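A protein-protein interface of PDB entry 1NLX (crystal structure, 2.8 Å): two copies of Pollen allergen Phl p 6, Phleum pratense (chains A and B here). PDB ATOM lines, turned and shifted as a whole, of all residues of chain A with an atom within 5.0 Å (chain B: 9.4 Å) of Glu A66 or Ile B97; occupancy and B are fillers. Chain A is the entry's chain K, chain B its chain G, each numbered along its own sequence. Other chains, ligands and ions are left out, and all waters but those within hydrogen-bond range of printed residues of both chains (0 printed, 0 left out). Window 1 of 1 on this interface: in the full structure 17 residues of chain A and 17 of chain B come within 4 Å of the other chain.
OE2 of Glu A66 sits close to N of Thr B101 (3.3 Å).
The side-chain carboxylate of Glu A66 sits close to the backbone carbonyl oxygen of Ile B97, at 3.4 Å.
The side-chain carboxylate (OE2) of Glu A66 lies close to the backbone carbonyl oxygen (O) of Gly B100 (3.3 Å).
N of Pro B102 lies close to OE2 of Glu A66, at 3.2 Å.
OE1 of Glu B66 sits close to O of Ile A97 (3.3 Å).
The backbone NH (N) of Thr B101 is in hydrogen-bond range of the backbone carbonyl oxygen (O) of Arg B96 (2.8 Å).
The guanidinium group (NH2) of Arg B96 sits at hydrogen-bond distance from the backbone carbonyl oxygen (O) of Val B104 (3.0 Å).
The backbone carbonyl oxygen of Asp A65 sits at hydrogen-bond distance from the side-chain amide nitrogen of Asn A69, 2.8 Å away.
O of Arg B96 touches OE1 of Glu A66, 3.8 Å away.
Pro B102 touches Asn A69 (O to O, 3.8 Å).
O of Pro B102 touches N of Ala A70 (3.9 Å).
CB of Ala A70 touches CG1 of Val B104 (3.2 Å).
Ile B97 touches Ala A94 (CD1 to CB, 3.5 Å).
CD1 of Ile A97 touches CB of Ala B94 (3.4 Å).
Ile A97 touches Ile B97.
Ile A97 touches Ile B98.
CG2 of Ile B97 touches CD1 of Ile A98, 3.3 Å away.
Asp A65 touches none of the printed residues of chain B.
Glu A66 touches just these residues of chain B: Arg B96, Ile B97, Gly B100, Thr B101 and Pro B102.
Ala A94 touches just one residue of chain B: Ile B97.
His B90 touches none of the printed residues of chain A.
Of the printed residues of chain A, Arg B96 touches Glu A66 (3.8 Å).
Ala B99 touches none of the printed residues of chain A.
Of the printed residues of chain A, Gly B100 touches Glu A66 (3.1 Å).
Of the printed residues of chain A, Thr B101 touches Glu A66.
Of the printed residues of chain A, Val B104 touches Ala A70 (3.2 Å).
Of the 24 printed residues of chain B, 9 touch a printed residue of chain A.
Of the 14 printed residues of chain A, 6 touch a printed residue of chain B.
Hydrophobic or aromatic side chains of chain A that line the printed part of chain B: Ala A70, Ala A94, Ile A97 and Ile A98.
Glu A66 touches Ile B97, and with the chains exchanged Ile A97 touches Glu B66.
Ala A94 touches Ile B97, and with the chains exchanged Ile A97 touches Ala B94.
Ile B97 touches its own counterpart, Ile A97.
Ile A97 touches Ile B98, and with the chains exchanged Ile A98 touches Ile B97.
Positions printed for both chains: 63, 66, 67, 70, 94, 97 and 98.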
ATOM      1  N   VAL A  61       4.302  -4.347 -22.376  1.00  0.00           N
ATOM      2  CA  VAL A  61       5.443  -5.203 -22.649  1.00  0.00           C
ATOM      3  C   VAL A  61       6.749  -4.706 -22.079  1.00  0.00           C
ATOM      4  O   VAL A  61       7.389  -5.402 -21.314  1.00  0.00           O
ATOM      5  CB  VAL A  61       5.622  -5.442 -24.160  1.00  0.00           C
ATOM      6  CG1 VAL A  61       6.900  -6.234 -24.427  1.00  0.00           C
ATOM      7  CG2 VAL A  61       4.428  -6.227 -24.690  1.00  0.00           C
ATOM      8  N   PRO A  62       7.167  -3.497 -22.438  1.00  0.00           N
ATOM      9  CA  PRO A  62       8.435  -3.003 -21.897  1.00  0.00           C
ATOM     10  C   PRO A  62       8.455  -2.940 -20.371  1.00  0.00           C
ATOM     11  O   PRO A  62       9.512  -3.141 -19.749  1.00  0.00           O
ATOM     12  CB  PRO A  62       8.586  -1.638 -22.557  1.00  0.00           C
ATOM     13  CG  PRO A  62       7.173  -1.207 -22.717  1.00  0.00           C
ATOM     14  CD  PRO A  62       6.488  -2.457 -23.220  1.00  0.00           C
ATOM     15  N   LYS A  63       7.301  -2.671 -19.766  1.00  0.00           N
ATOM     16  CA  LYS A  63       7.234  -2.617 -18.310  1.00  0.00           C
ATOM     17  C   LYS A  63       7.496  -4.007 -17.781  1.00  0.00           C
ATOM     18  O   LYS A  63       8.309  -4.202 -16.888  1.00  0.00           O
ATOM     19  CB  LYS A  63       5.867  -2.138 -17.838  1.00  0.00           C
ATOM     20  CG  LYS A  63       5.591  -0.665 -18.122  1.00  0.00           C
ATOM     21  CD  LYS A  63       4.196  -0.295 -17.676  1.00  0.00           C
ATOM     22  CE  LYS A  63       3.803   1.094 -18.157  1.00  0.00           C
ATOM     23  NZ  LYS A  63       2.424   1.433 -17.691  1.00  0.00           N
ATOM     24  N   LEU A  64       6.808  -4.982 -18.353  1.00  0.00           N
ATOM     25  CA  LEU A  64       6.966  -6.385 -17.976  1.00  0.00           C
ATOM     26  C   LEU A  64       8.422  -6.824 -18.139  1.00  0.00           C
ATOM     27  O   LEU A  64       8.963  -7.507 -17.278  1.00  0.00           O
ATOM     28  CB  LEU A  64       6.050  -7.249 -18.844  1.00  0.00           C
ATOM     29  CG  LEU A  64       4.993  -8.077 -18.116  1.00  0.00           C
ATOM     30  CD1 LEU A  64       4.444  -7.346 -16.919  1.00  0.00           C
ATOM     31  CD2 LEU A  64       3.885  -8.404 -19.089  1.00  0.00           C
ATOM     32  N   ASP A  65       9.047  -6.423 -19.245  1.00  0.00           N
ATOM     33  CA  ASP A  65      10.440  -6.749 -19.531  1.00  0.00           C
ATOM     34  C   ASP A  65      11.296  -6.215 -18.383  1.00  0.00           C
ATOM     35  O   ASP A  65      12.287  -6.836 -17.985  1.00  0.00           O
ATOM     36  CB  ASP A  65      10.859  -6.103 -20.862  1.00  0.00           C
ATOM     37  CG  ASP A  65      12.238  -6.567 -21.340  1.00  0.00           C
ATOM     38  OD1 ASP A  65      12.432  -7.801 -21.461  1.00  0.00           O
ATOM     39  OD2 ASP A  65      13.126  -5.708 -21.601  1.00  0.00           O
ATOM     40  N   GLU A  66      10.887  -5.060 -17.852  1.00  0.00           N
ATOM     41  CA  GLU A  66      11.573  -4.407 -16.739  1.00  0.00           C
ATOM     42  C   GLU A  66      11.506  -5.200 -15.437  1.00  0.00           C
ATOM     43  O   GLU A  66      12.522  -5.376 -14.771  1.00  0.00           O
ATOM     44  CB  GLU A  66      10.974  -3.031 -16.469  1.00  0.00           C
ATOM     45  CG  GLU A  66      11.953  -1.865 -16.573  1.00  0.00           C
ATOM     46  CD  GLU A  66      13.126  -1.923 -15.596  1.00  0.00           C
ATOM     47  OE1 GLU A  66      12.912  -1.778 -14.376  1.00  0.00           O
ATOM     48  OE2 GLU A  66      14.272  -2.101 -16.056  1.00  0.00           O
ATOM     49  N   VAL A  67      10.320  -5.668 -15.053  1.00  0.00           N
ATOM     50  CA  VAL A  67      10.240  -6.380 -13.793  1.00  0.00           C
ATOM     51  C   VAL A  67      10.961  -7.686 -13.938  1.00  0.00           C
ATOM     52  O   VAL A  67      11.650  -8.109 -13.019  1.00  0.00           O
ATOM     53  CB  VAL A  67       8.780  -6.622 -13.306  1.00  0.00           C
ATOM     54  CG1 VAL A  67       7.809  -5.790 -14.116  1.00  0.00           C
ATOM     55  CG2 VAL A  67       8.437  -8.103 -13.345  1.00  0.00           C
ATOM     56  N   TYR A  68      10.817  -8.327 -15.091  1.00  0.00           N
ATOM     57  CA  TYR A  68      11.518  -9.586 -15.300  1.00  0.00           C
ATOM     58  C   TYR A  68      13.003  -9.278 -15.159  1.00  0.00           C
ATOM     59  O   TYR A  68      13.733 -10.005 -14.474  1.00  0.00           O
ATOM     60  CB  TYR A  68      11.270 -10.154 -16.699  1.00  0.00           C
ATOM     61  CG  TYR A  68       9.915 -10.786 -16.951  1.00  0.00           C
ATOM     62  CD1 TYR A  68       9.456 -10.959 -18.263  1.00  0.00           C
ATOM     63  CD2 TYR A  68       9.105 -11.226 -15.907  1.00  0.00           C
ATOM     64  CE1 TYR A  68       8.229 -11.550 -18.532  1.00  0.00           C
ATOM     65  CE2 TYR A  68       7.867 -11.825 -16.163  1.00  0.00           C
ATOM     66  CZ  TYR A  68       7.438 -11.981 -17.484  1.00  0.00           C
ATOM     67  OH  TYR A  68       6.217 -12.562 -17.774  1.00  0.00           O
ATOM     68  N   ASN A  69      13.442  -8.195 -15.804  1.00  0.00           N
ATOM     69  CA  ASN A  69      14.845  -7.817 -15.748  1.00  0.00           C
ATOM     70  C   ASN A  69      15.272  -7.567 -14.312  1.00  0.00           C
ATOM     71  O   ASN A  69      16.311  -8.062 -13.865  1.00  0.00           O
ATOM     72  CB  ASN A  69      15.112  -6.576 -16.586  1.00  0.00           C
ATOM     73  CG  ASN A  69      15.373  -6.903 -18.041  1.00  0.00           C
ATOM     74  OD1 ASN A  69      16.102  -7.844 -18.350  1.00  0.00           O
ATOM     75  ND2 ASN A  69      14.789  -6.121 -18.943  1.00  0.00           N
ATOM     76  N   ALA A  70      14.461  -6.798 -13.593  1.00  0.00           N
ATOM     77  CA  ALA A  70      14.727  -6.484 -12.203  1.00  0.00           C
ATOM     78  C   ALA A  70      15.002  -7.774 -11.432  1.00  0.00           C
ATOM     79  O   ALA A  70      16.021  -7.893 -10.739  1.00  0.00           O
ATOM     80  CB  ALA A  70      13.532  -5.768 -11.603  1.00  0.00           C
ATOM     81  N   ALA A  71      14.092  -8.739 -11.564  1.00  0.00           N
ATOM     82  CA  ALA A  71      14.226 -10.010 -10.861  1.00  0.00           C
ATOM     83  C   ALA A  71      15.419 -10.845 -11.311  1.00  0.00           C
ATOM     84  O   ALA A  71      16.234 -11.253 -10.481  1.00  0.00           O
ATOM     85  CB  ALA A  71      12.944 -10.834 -10.986  1.00  0.00           C
ATOM     86  N   ALA A  94       8.694  -5.265  -7.868  1.00  0.00           N
ATOM     87  CA  ALA A  94       8.698  -4.610  -9.164  1.00  0.00           C
ATOM     88  C   ALA A  94       7.334  -4.703  -9.833  1.00  0.00           C
ATOM     89  O   ALA A  94       6.880  -3.756 -10.471  1.00  0.00           O
ATOM     90  CB  ALA A  94       9.760  -5.226 -10.055  1.00  0.00           C
ATOM     91  N   ILE A  97       4.956  -2.281  -8.258  1.00  0.00           N
ATOM     92  CA  ILE A  97       5.215  -0.929  -8.693  1.00  0.00           C
ATOM     93  C   ILE A  97       4.574  -0.717 -10.051  1.00  0.00           C
ATOM     94  O   ILE A  97       3.824   0.240 -10.267  1.00  0.00           O
ATOM     95  CB  ILE A  97       6.710  -0.681  -8.768  1.00  0.00           C
ATOM     96  CG1 ILE A  97       7.242  -0.487  -7.348  1.00  0.00           C
ATOM     97  CG2 ILE A  97       7.008   0.499  -9.654  1.00  0.00           C
ATOM     98  CD1 ILE A  97       8.751  -0.434  -7.243  1.00  0.00           C
ATOM     99  N   ILE A  98       4.857  -1.631 -10.967  1.00  0.00           N
ATOM    100  CA  ILE A  98       4.306  -1.535 -12.307  1.00  0.00           C
ATOM    101  C   ILE A  98       2.785  -1.511 -12.248  1.00  0.00           C
ATOM    102  O   ILE A  98       2.142  -0.872 -13.066  1.00  0.00           O
ATOM    103  CB  ILE A  98       4.823  -2.713 -13.191  1.00  0.00           C
ATOM    104  CG1 ILE A  98       5.827  -2.178 -14.196  1.00  0.00           C
ATOM    105  CG2 ILE A  98       3.704  -3.417 -13.923  1.00  0.00           C
ATOM    106  CD1 ILE A  98       6.995  -1.490 -13.538  1.00  0.00           C
ATOM    107  N   GLU B   8      10.285  13.024 -20.080  1.00  0.00           N
ATOM    108  CA  GLU B   8      10.150  12.055 -19.011  1.00  0.00           C
ATOM    109  C   GLU B   8      11.521  11.707 -18.443  1.00  0.00           C
ATOM    110  O   GLU B   8      11.704  11.709 -17.235  1.00  0.00           O
ATOM    111  CB  GLU B   8       9.465  10.806 -19.546  1.00  0.00           C
ATOM    112  CG  GLU B   8       8.785   9.970 -18.481  1.00  0.00           C
ATOM    113  CD  GLU B   8       7.892   8.891 -19.076  1.00  0.00           C
ATOM    114  OE1 GLU B   8       7.000   9.244 -19.888  1.00  0.00           O
ATOM    115  OE2 GLU B   8       8.075   7.699 -18.732  1.00  0.00           O
ATOM    116  N   ILE B  12      13.008  12.385 -14.608  1.00  0.00           N
ATOM    117  CA  ILE B  12      13.499  11.333 -13.729  1.00  0.00           C
ATOM    118  C   ILE B  12      14.844  11.783 -13.169  1.00  0.00           C
ATOM    119  O   ILE B  12      15.135  11.568 -11.997  1.00  0.00           O
ATOM    120  CB  ILE B  12      13.720   9.998 -14.473  1.00  0.00           C
ATOM    121  CG1 ILE B  12      12.458   9.582 -15.234  1.00  0.00           C
ATOM    122  CG2 ILE B  12      14.105   8.914 -13.471  1.00  0.00           C
ATOM    123  CD1 ILE B  12      11.321   9.111 -14.372  1.00  0.00           C
ATOM    124  N   LEU B  60       3.885  10.616 -16.549  1.00  0.00           N
ATOM    125  CA  LEU B  60       4.887  10.281 -15.552  1.00  0.00           C
ATOM    126  C   LEU B  60       4.424  10.555 -14.117  1.00  0.00           C
ATOM    127  O   LEU B  60       4.970   9.992 -13.161  1.00  0.00           O
ATOM    128  CB  LEU B  60       6.169  11.060 -15.845  1.00  0.00           C
ATOM    129  CG  LEU B  60       7.330  10.887 -14.865  1.00  0.00           C
ATOM    130  CD1 LEU B  60       7.816   9.461 -14.906  1.00  0.00           C
ATOM    131  CD2 LEU B  60       8.455  11.829 -15.226  1.00  0.00           C
ATOM    132  N   LYS B  63       3.195   7.503 -12.124  1.00  0.00           N
ATOM    133  CA  LYS B  63       4.320   6.613 -11.875  1.00  0.00           C
ATOM    134  C   LYS B  63       5.115   7.179 -10.716  1.00  0.00           C
ATOM    135  O   LYS B  63       5.460   6.466  -9.784  1.00  0.00           O
ATOM    136  CB  LYS B  63       5.219   6.506 -13.107  1.00  0.00           C
ATOM    137  CG  LYS B  63       4.597   5.757 -14.284  1.00  0.00           C
ATOM    138  CD  LYS B  63       5.532   5.772 -15.474  1.00  0.00           C
ATOM    139  CE  LYS B  63       4.853   5.217 -16.704  1.00  0.00           C
ATOM    140  NZ  LYS B  63       5.801   5.204 -17.862  1.00  0.00           N
ATOM    141  N   GLU B  66       3.645   6.635  -7.499  1.00  0.00           N
ATOM    142  CA  GLU B  66       3.869   5.265  -7.050  1.00  0.00           C
ATOM    143  C   GLU B  66       5.187   5.125  -6.319  1.00  0.00           C
ATOM    144  O   GLU B  66       5.243   4.577  -5.222  1.00  0.00           O
ATOM    145  CB  GLU B  66       3.868   4.307  -8.234  1.00  0.00           C
ATOM    146  CG  GLU B  66       2.882   3.169  -8.116  1.00  0.00           C
ATOM    147  CD  GLU B  66       3.208   2.197  -7.006  1.00  0.00           C
ATOM    148  OE1 GLU B  66       4.145   1.387  -7.147  1.00  0.00           O
ATOM    149  OE2 GLU B  66       2.517   2.248  -5.976  1.00  0.00           O
ATOM    150  N   VAL B  67       6.253   5.621  -6.927  1.00  0.00           N
ATOM    151  CA  VAL B  67       7.556   5.508  -6.303  1.00  0.00           C
ATOM    152  C   VAL B  67       7.511   6.195  -4.960  1.00  0.00           C
ATOM    153  O   VAL B  67       7.965   5.648  -3.965  1.00  0.00           O
ATOM    154  CB  VAL B  67       8.663   6.141  -7.167  1.00  0.00           C
ATOM    155  CG1 VAL B  67       8.831   5.374  -8.471  1.00  0.00           C
ATOM    156  CG2 VAL B  67       8.305   7.542  -7.470  1.00  0.00           C
ATOM    157  N   ALA B  70       5.661   4.054  -2.654  1.00  0.00           N
ATOM    158  CA  ALA B  70       6.496   2.895  -2.372  1.00  0.00           C
ATOM    159  C   ALA B  70       7.429   3.166  -1.190  1.00  0.00           C
ATOM    160  O   ALA B  70       7.450   2.405  -0.222  1.00  0.00           O
ATOM    161  CB  ALA B  70       7.307   2.538  -3.593  1.00  0.00           C
ATOM    162  N   LEU B  89      16.233   2.787   0.102  1.00  0.00           N
ATOM    163  CA  LEU B  89      16.308   1.545  -0.649  1.00  0.00           C
ATOM    164  C   LEU B  89      15.143   1.393  -1.616  1.00  0.00           C
ATOM    165  O   LEU B  89      15.343   1.164  -2.809  1.00  0.00           O
ATOM    166  CB  LEU B  89      16.324   0.362   0.307  1.00  0.00           C
ATOM    167  CG  LEU B  89      16.291  -0.992  -0.388  1.00  0.00           C
ATOM    168  CD1 LEU B  89      17.476  -1.091  -1.343  1.00  0.00           C
ATOM    169  CD2 LEU B  89      16.328  -2.112   0.666  1.00  0.00           C
ATOM    170  N   HIS B  90      13.922   1.527  -1.104  1.00  0.00           N
ATOM    171  CA  HIS B  90      12.753   1.373  -1.947  1.00  0.00           C
ATOM    172  C   HIS B  90      12.564   2.484  -2.964  1.00  0.00           C
ATOM    173  O   HIS B  90      12.039   2.255  -4.056  1.00  0.00           O
ATOM    174  CB  HIS B  90      11.500   1.210  -1.088  1.00  0.00           C
ATOM    175  CG  HIS B  90      11.397  -0.134  -0.444  1.00  0.00           C
ATOM    176  ND1 HIS B  90      12.097  -0.471   0.695  1.00  0.00           N
ATOM    177  CD2 HIS B  90      10.741  -1.257  -0.828  1.00  0.00           C
ATOM    178  CE1 HIS B  90      11.881  -1.742   0.984  1.00  0.00           C
ATOM    179  NE2 HIS B  90      11.062  -2.242   0.074  1.00  0.00           N
ATOM    180  N   PHE B  91      13.002   3.684  -2.628  1.00  0.00           N
ATOM    181  CA  PHE B  91      12.855   4.780  -3.553  1.00  0.00           C
ATOM    182  C   PHE B  91      13.794   4.607  -4.743  1.00  0.00           C
ATOM    183  O   PHE B  91      13.373   4.678  -5.897  1.00  0.00           O
ATOM    184  CB  PHE B  91      13.169   6.093  -2.856  1.00  0.00           C
ATOM    185  CG  PHE B  91      12.916   7.296  -3.711  1.00  0.00           C
ATOM    186  CD1 PHE B  91      11.658   7.892  -3.737  1.00  0.00           C
ATOM    187  CD2 PHE B  91      13.924   7.808  -4.530  1.00  0.00           C
ATOM    188  CE1 PHE B  91      11.405   8.979  -4.567  1.00  0.00           C
ATOM    189  CE2 PHE B  91      13.681   8.892  -5.363  1.00  0.00           C
ATOM    190  CZ  PHE B  91      12.414   9.482  -5.383  1.00  0.00           C
ATOM    191  N   SER B  92      15.074   4.393  -4.458  1.00  0.00           N
ATOM    192  CA  SER B  92      16.051   4.231  -5.520  1.00  0.00           C
ATOM    193  C   SER B  92      15.654   3.104  -6.466  1.00  0.00           C
ATOM    194  O   SER B  92      15.720   3.272  -7.679  1.00  0.00           O
ATOM    195  CB  SER B  92      17.436   3.960  -4.948  1.00  0.00           C
ATOM    196  OG  SER B  92      17.472   2.701  -4.329  1.00  0.00           O
ATOM    197  N   GLU B  93      15.233   1.961  -5.930  1.00  0.00           N
ATOM    198  CA  GLU B  93      14.840   0.855  -6.798  1.00  0.00           C
ATOM    199  C   GLU B  93      13.570   1.181  -7.577  1.00  0.00           C
ATOM    200  O   GLU B  93      13.525   1.010  -8.796  1.00  0.00           O
ATOM    201  CB  GLU B  93      14.670  -0.448  -5.995  1.00  0.00           C
ATOM    202  CG  GLU B  93      16.022  -1.015  -5.537  1.00  0.00           C
ATOM    203  CD  GLU B  93      15.973  -2.420  -4.926  1.00  0.00           C
ATOM    204  OE1 GLU B  93      17.081  -2.950  -4.659  1.00  0.00           O
ATOM    205  OE2 GLU B  93      14.860  -2.981  -4.713  1.00  0.00           O
ATOM    206  N   ALA B  94      12.550   1.680  -6.887  1.00  0.00           N
ATOM    207  CA  ALA B  94      11.300   2.008  -7.560  1.00  0.00           C
ATOM    208  C   ALA B  94      11.540   2.995  -8.691  1.00  0.00           C
ATOM    209  O   ALA B  94      10.942   2.876  -9.763  1.00  0.00           O
ATOM    210  CB  ALA B  94      10.300   2.569  -6.577  1.00  0.00           C
ATOM    211  N   LEU B  95      12.420   3.962  -8.464  1.00  0.00           N
ATOM    212  CA  LEU B  95      12.712   4.940  -9.495  1.00  0.00           C
ATOM    213  C   LEU B  95      13.414   4.270 -10.676  1.00  0.00           C
ATOM    214  O   LEU B  95      13.139   4.593 -11.833  1.00  0.00           O
ATOM    215  CB  LEU B  95      13.589   6.064  -8.942  1.00  0.00           C
ATOM    216  CG  LEU B  95      13.678   7.261  -9.890  1.00  0.00           C
ATOM    217  CD1 LEU B  95      12.303   7.873 -10.092  1.00  0.00           C
ATOM    218  CD2 LEU B  95      14.619   8.286  -9.324  1.00  0.00           C
ATOM    219  N   ARG B  96      14.322   3.338 -10.394  1.00  0.00           N
ATOM    220  CA  ARG B  96      15.024   2.644 -11.468  1.00  0.00           C
ATOM    221  C   ARG B  96      14.035   1.836 -12.309  1.00  0.00           C
ATOM    222  O   ARG B  96      14.154   1.767 -13.536  1.00  0.00           O
ATOM    223  CB  ARG B  96      16.099   1.723 -10.902  1.00  0.00           C
ATOM    224  CG  ARG B  96      17.432   2.405 -10.730  1.00  0.00           C
ATOM    225  CD  ARG B  96      18.341   1.571  -9.890  1.00  0.00           C
ATOM    226  NE  ARG B  96      19.131   2.417  -9.016  1.00  0.00           N
ATOM    227  CZ  ARG B  96      19.473   2.084  -7.775  1.00  0.00           C
ATOM    228  NH1 ARG B  96      20.200   2.915  -7.034  1.00  0.00           N
ATOM    229  NH2 ARG B  96      19.082   0.919  -7.271  1.00  0.00           N
ATOM    230  N   ILE B  97      13.059   1.230 -11.646  1.00  0.00           N
ATOM    231  CA  ILE B  97      12.062   0.463 -12.350  1.00  0.00           C
ATOM    232  C   ILE B  97      11.266   1.379 -13.260  1.00  0.00           C
ATOM    233  O   ILE B  97      11.092   1.099 -14.451  1.00  0.00           O
ATOM    234  CB  ILE B  97      11.124  -0.233 -11.365  1.00  0.00           C
ATOM    235  CG1 ILE B  97      11.857  -1.446 -10.778  1.00  0.00           C
ATOM    236  CG2 ILE B  97       9.828  -0.626 -12.049  1.00  0.00           C
ATOM    237  CD1 ILE B  97      11.147  -2.085  -9.628  1.00  0.00           C
ATOM    238  N   ILE B  98      10.783   2.480 -12.702  1.00  0.00           N
ATOM    239  CA  ILE B  98      10.009   3.431 -13.472  1.00  0.00           C
ATOM    240  C   ILE B  98      10.828   3.949 -14.643  1.00  0.00           C
ATOM    241  O   ILE B  98      10.276   4.220 -15.718  1.00  0.00           O
ATOM    242  CB  ILE B  98       9.537   4.584 -12.559  1.00  0.00           C
ATOM    243  CG1 ILE B  98       8.041   4.437 -12.328  1.00  0.00           C
ATOM    244  CG2 ILE B  98       9.834   5.943 -13.151  1.00  0.00           C
ATOM    245  CD1 ILE B  98       7.669   3.127 -11.722  1.00  0.00           C
ATOM    246  N   ALA B  99      12.144   4.055 -14.452  1.00  0.00           N
ATOM    247  CA  ALA B  99      13.031   4.554 -15.500  1.00  0.00           C
ATOM    248  C   ALA B  99      13.348   3.503 -16.579  1.00  0.00           C
ATOM    249  O   ALA B  99      13.871   3.823 -17.649  1.00  0.00           O
ATOM    250  CB  ALA B  99      14.306   5.044 -14.879  1.00  0.00           C
ATOM    251  N   GLY B 100      13.036   2.246 -16.307  1.00  0.00           N
ATOM    252  CA  GLY B 100      13.348   1.226 -17.284  1.00  0.00           C
ATOM    253  C   GLY B 100      14.793   0.784 -17.156  1.00  0.00           C
ATOM    254  O   GLY B 100      15.370   0.229 -18.080  1.00  0.00           O
ATOM    255  N   THR B 101      15.387   1.047 -16.000  1.00  0.00           N
ATOM    256  CA  THR B 101      16.760   0.636 -15.743  1.00  0.00           C
ATOM    257  C   THR B 101      16.765  -0.858 -15.382  1.00  0.00           C
ATOM    258  O   THR B 101      16.140  -1.285 -14.404  1.00  0.00           O
ATOM    259  CB  THR B 101      17.367   1.461 -14.596  1.00  0.00           C
ATOM    260  OG1 THR B 101      17.506   2.817 -15.019  1.00  0.00           O
ATOM    261  CG2 THR B 101      18.724   0.918 -14.202  1.00  0.00           C
ATOM    262  N   PRO B 102      17.474  -1.671 -16.173  1.00  0.00           N
ATOM    263  CA  PRO B 102      17.551  -3.114 -15.945  1.00  0.00           C
ATOM    264  C   PRO B 102      18.154  -3.580 -14.625  1.00  0.00           C
ATOM    265  O   PRO B 102      17.635  -4.521 -14.021  1.00  0.00           O
ATOM    266  CB  PRO B 102      18.336  -3.612 -17.158  1.00  0.00           C
ATOM    267  CG  PRO B 102      19.253  -2.478 -17.432  1.00  0.00           C
ATOM    268  CD  PRO B 102      18.318  -1.285 -17.312  1.00  0.00           C
ATOM    269  N   GLU B 103      19.239  -2.962 -14.173  1.00  0.00           N
ATOM    270  CA  GLU B 103      19.835  -3.399 -12.920  1.00  0.00           C
ATOM    271  C   GLU B 103      19.197  -2.573 -11.833  1.00  0.00           C
ATOM    272  O   GLU B 103      19.675  -1.488 -11.547  1.00  0.00           O
ATOM    273  CB  GLU B 103      21.348  -3.170 -12.922  1.00  0.00           C
ATOM    274  CG  GLU B 103      22.096  -3.928 -14.002  1.00  0.00           C
ATOM    275  CD  GLU B 103      22.698  -5.262 -13.539  1.00  0.00           C
ATOM    276  OE1 GLU B 103      22.116  -5.925 -12.643  1.00  0.00           O
ATOM    277  OE2 GLU B 103      23.758  -5.647 -14.097  1.00  0.00           O
ATOM    278  N   VAL B 104      18.124  -3.055 -11.215  1.00  0.00           N
ATOM    279  CA  VAL B 104      17.503  -2.248 -10.188  1.00  0.00           C
ATOM    280  C   VAL B 104      18.091  -2.443  -8.805  1.00  0.00           C
ATOM    281  O   VAL B 104      17.790  -1.661  -7.916  1.00  0.00           O
ATOM    282  CB  VAL B 104      15.956  -2.452 -10.139  1.00  0.00           C
ATOM    283  CG1 VAL B 104      15.508  -3.284 -11.306  1.00  0.00           C
ATOM    284  CG2 VAL B 104      15.523  -3.060  -8.832  1.00  0.00           C
ATOM    285  N   HIS B 105      18.951  -3.444  -8.609  1.00  0.00           N
ATOM    286  CA  HIS B 105      19.504  -3.650  -7.276  1.00  0.00           C
ATOM    287  C   HIS B 105      20.842  -2.981  -6.915  1.00  0.00           C
ATOM    288  O   HIS B 105      20.845  -2.018  -6.135  1.00  0.00           O
ATOM    289  CB  HIS B 105      19.588  -5.131  -6.942  1.00  0.00           C
ATOM    290  CG  HIS B 105      19.874  -5.392  -5.496  1.00  0.00           C
ATOM    291  ND1 HIS B 105      18.939  -5.189  -4.504  1.00  0.00           N
ATOM    292  CD2 HIS B 105      21.008  -5.791  -4.867  1.00  0.00           C
ATOM    293  CE1 HIS B 105      19.483  -5.450  -3.328  1.00  0.00           C
ATOM    294  NE2 HIS B 105      20.738  -5.818  -3.519  1.00  0.00           N
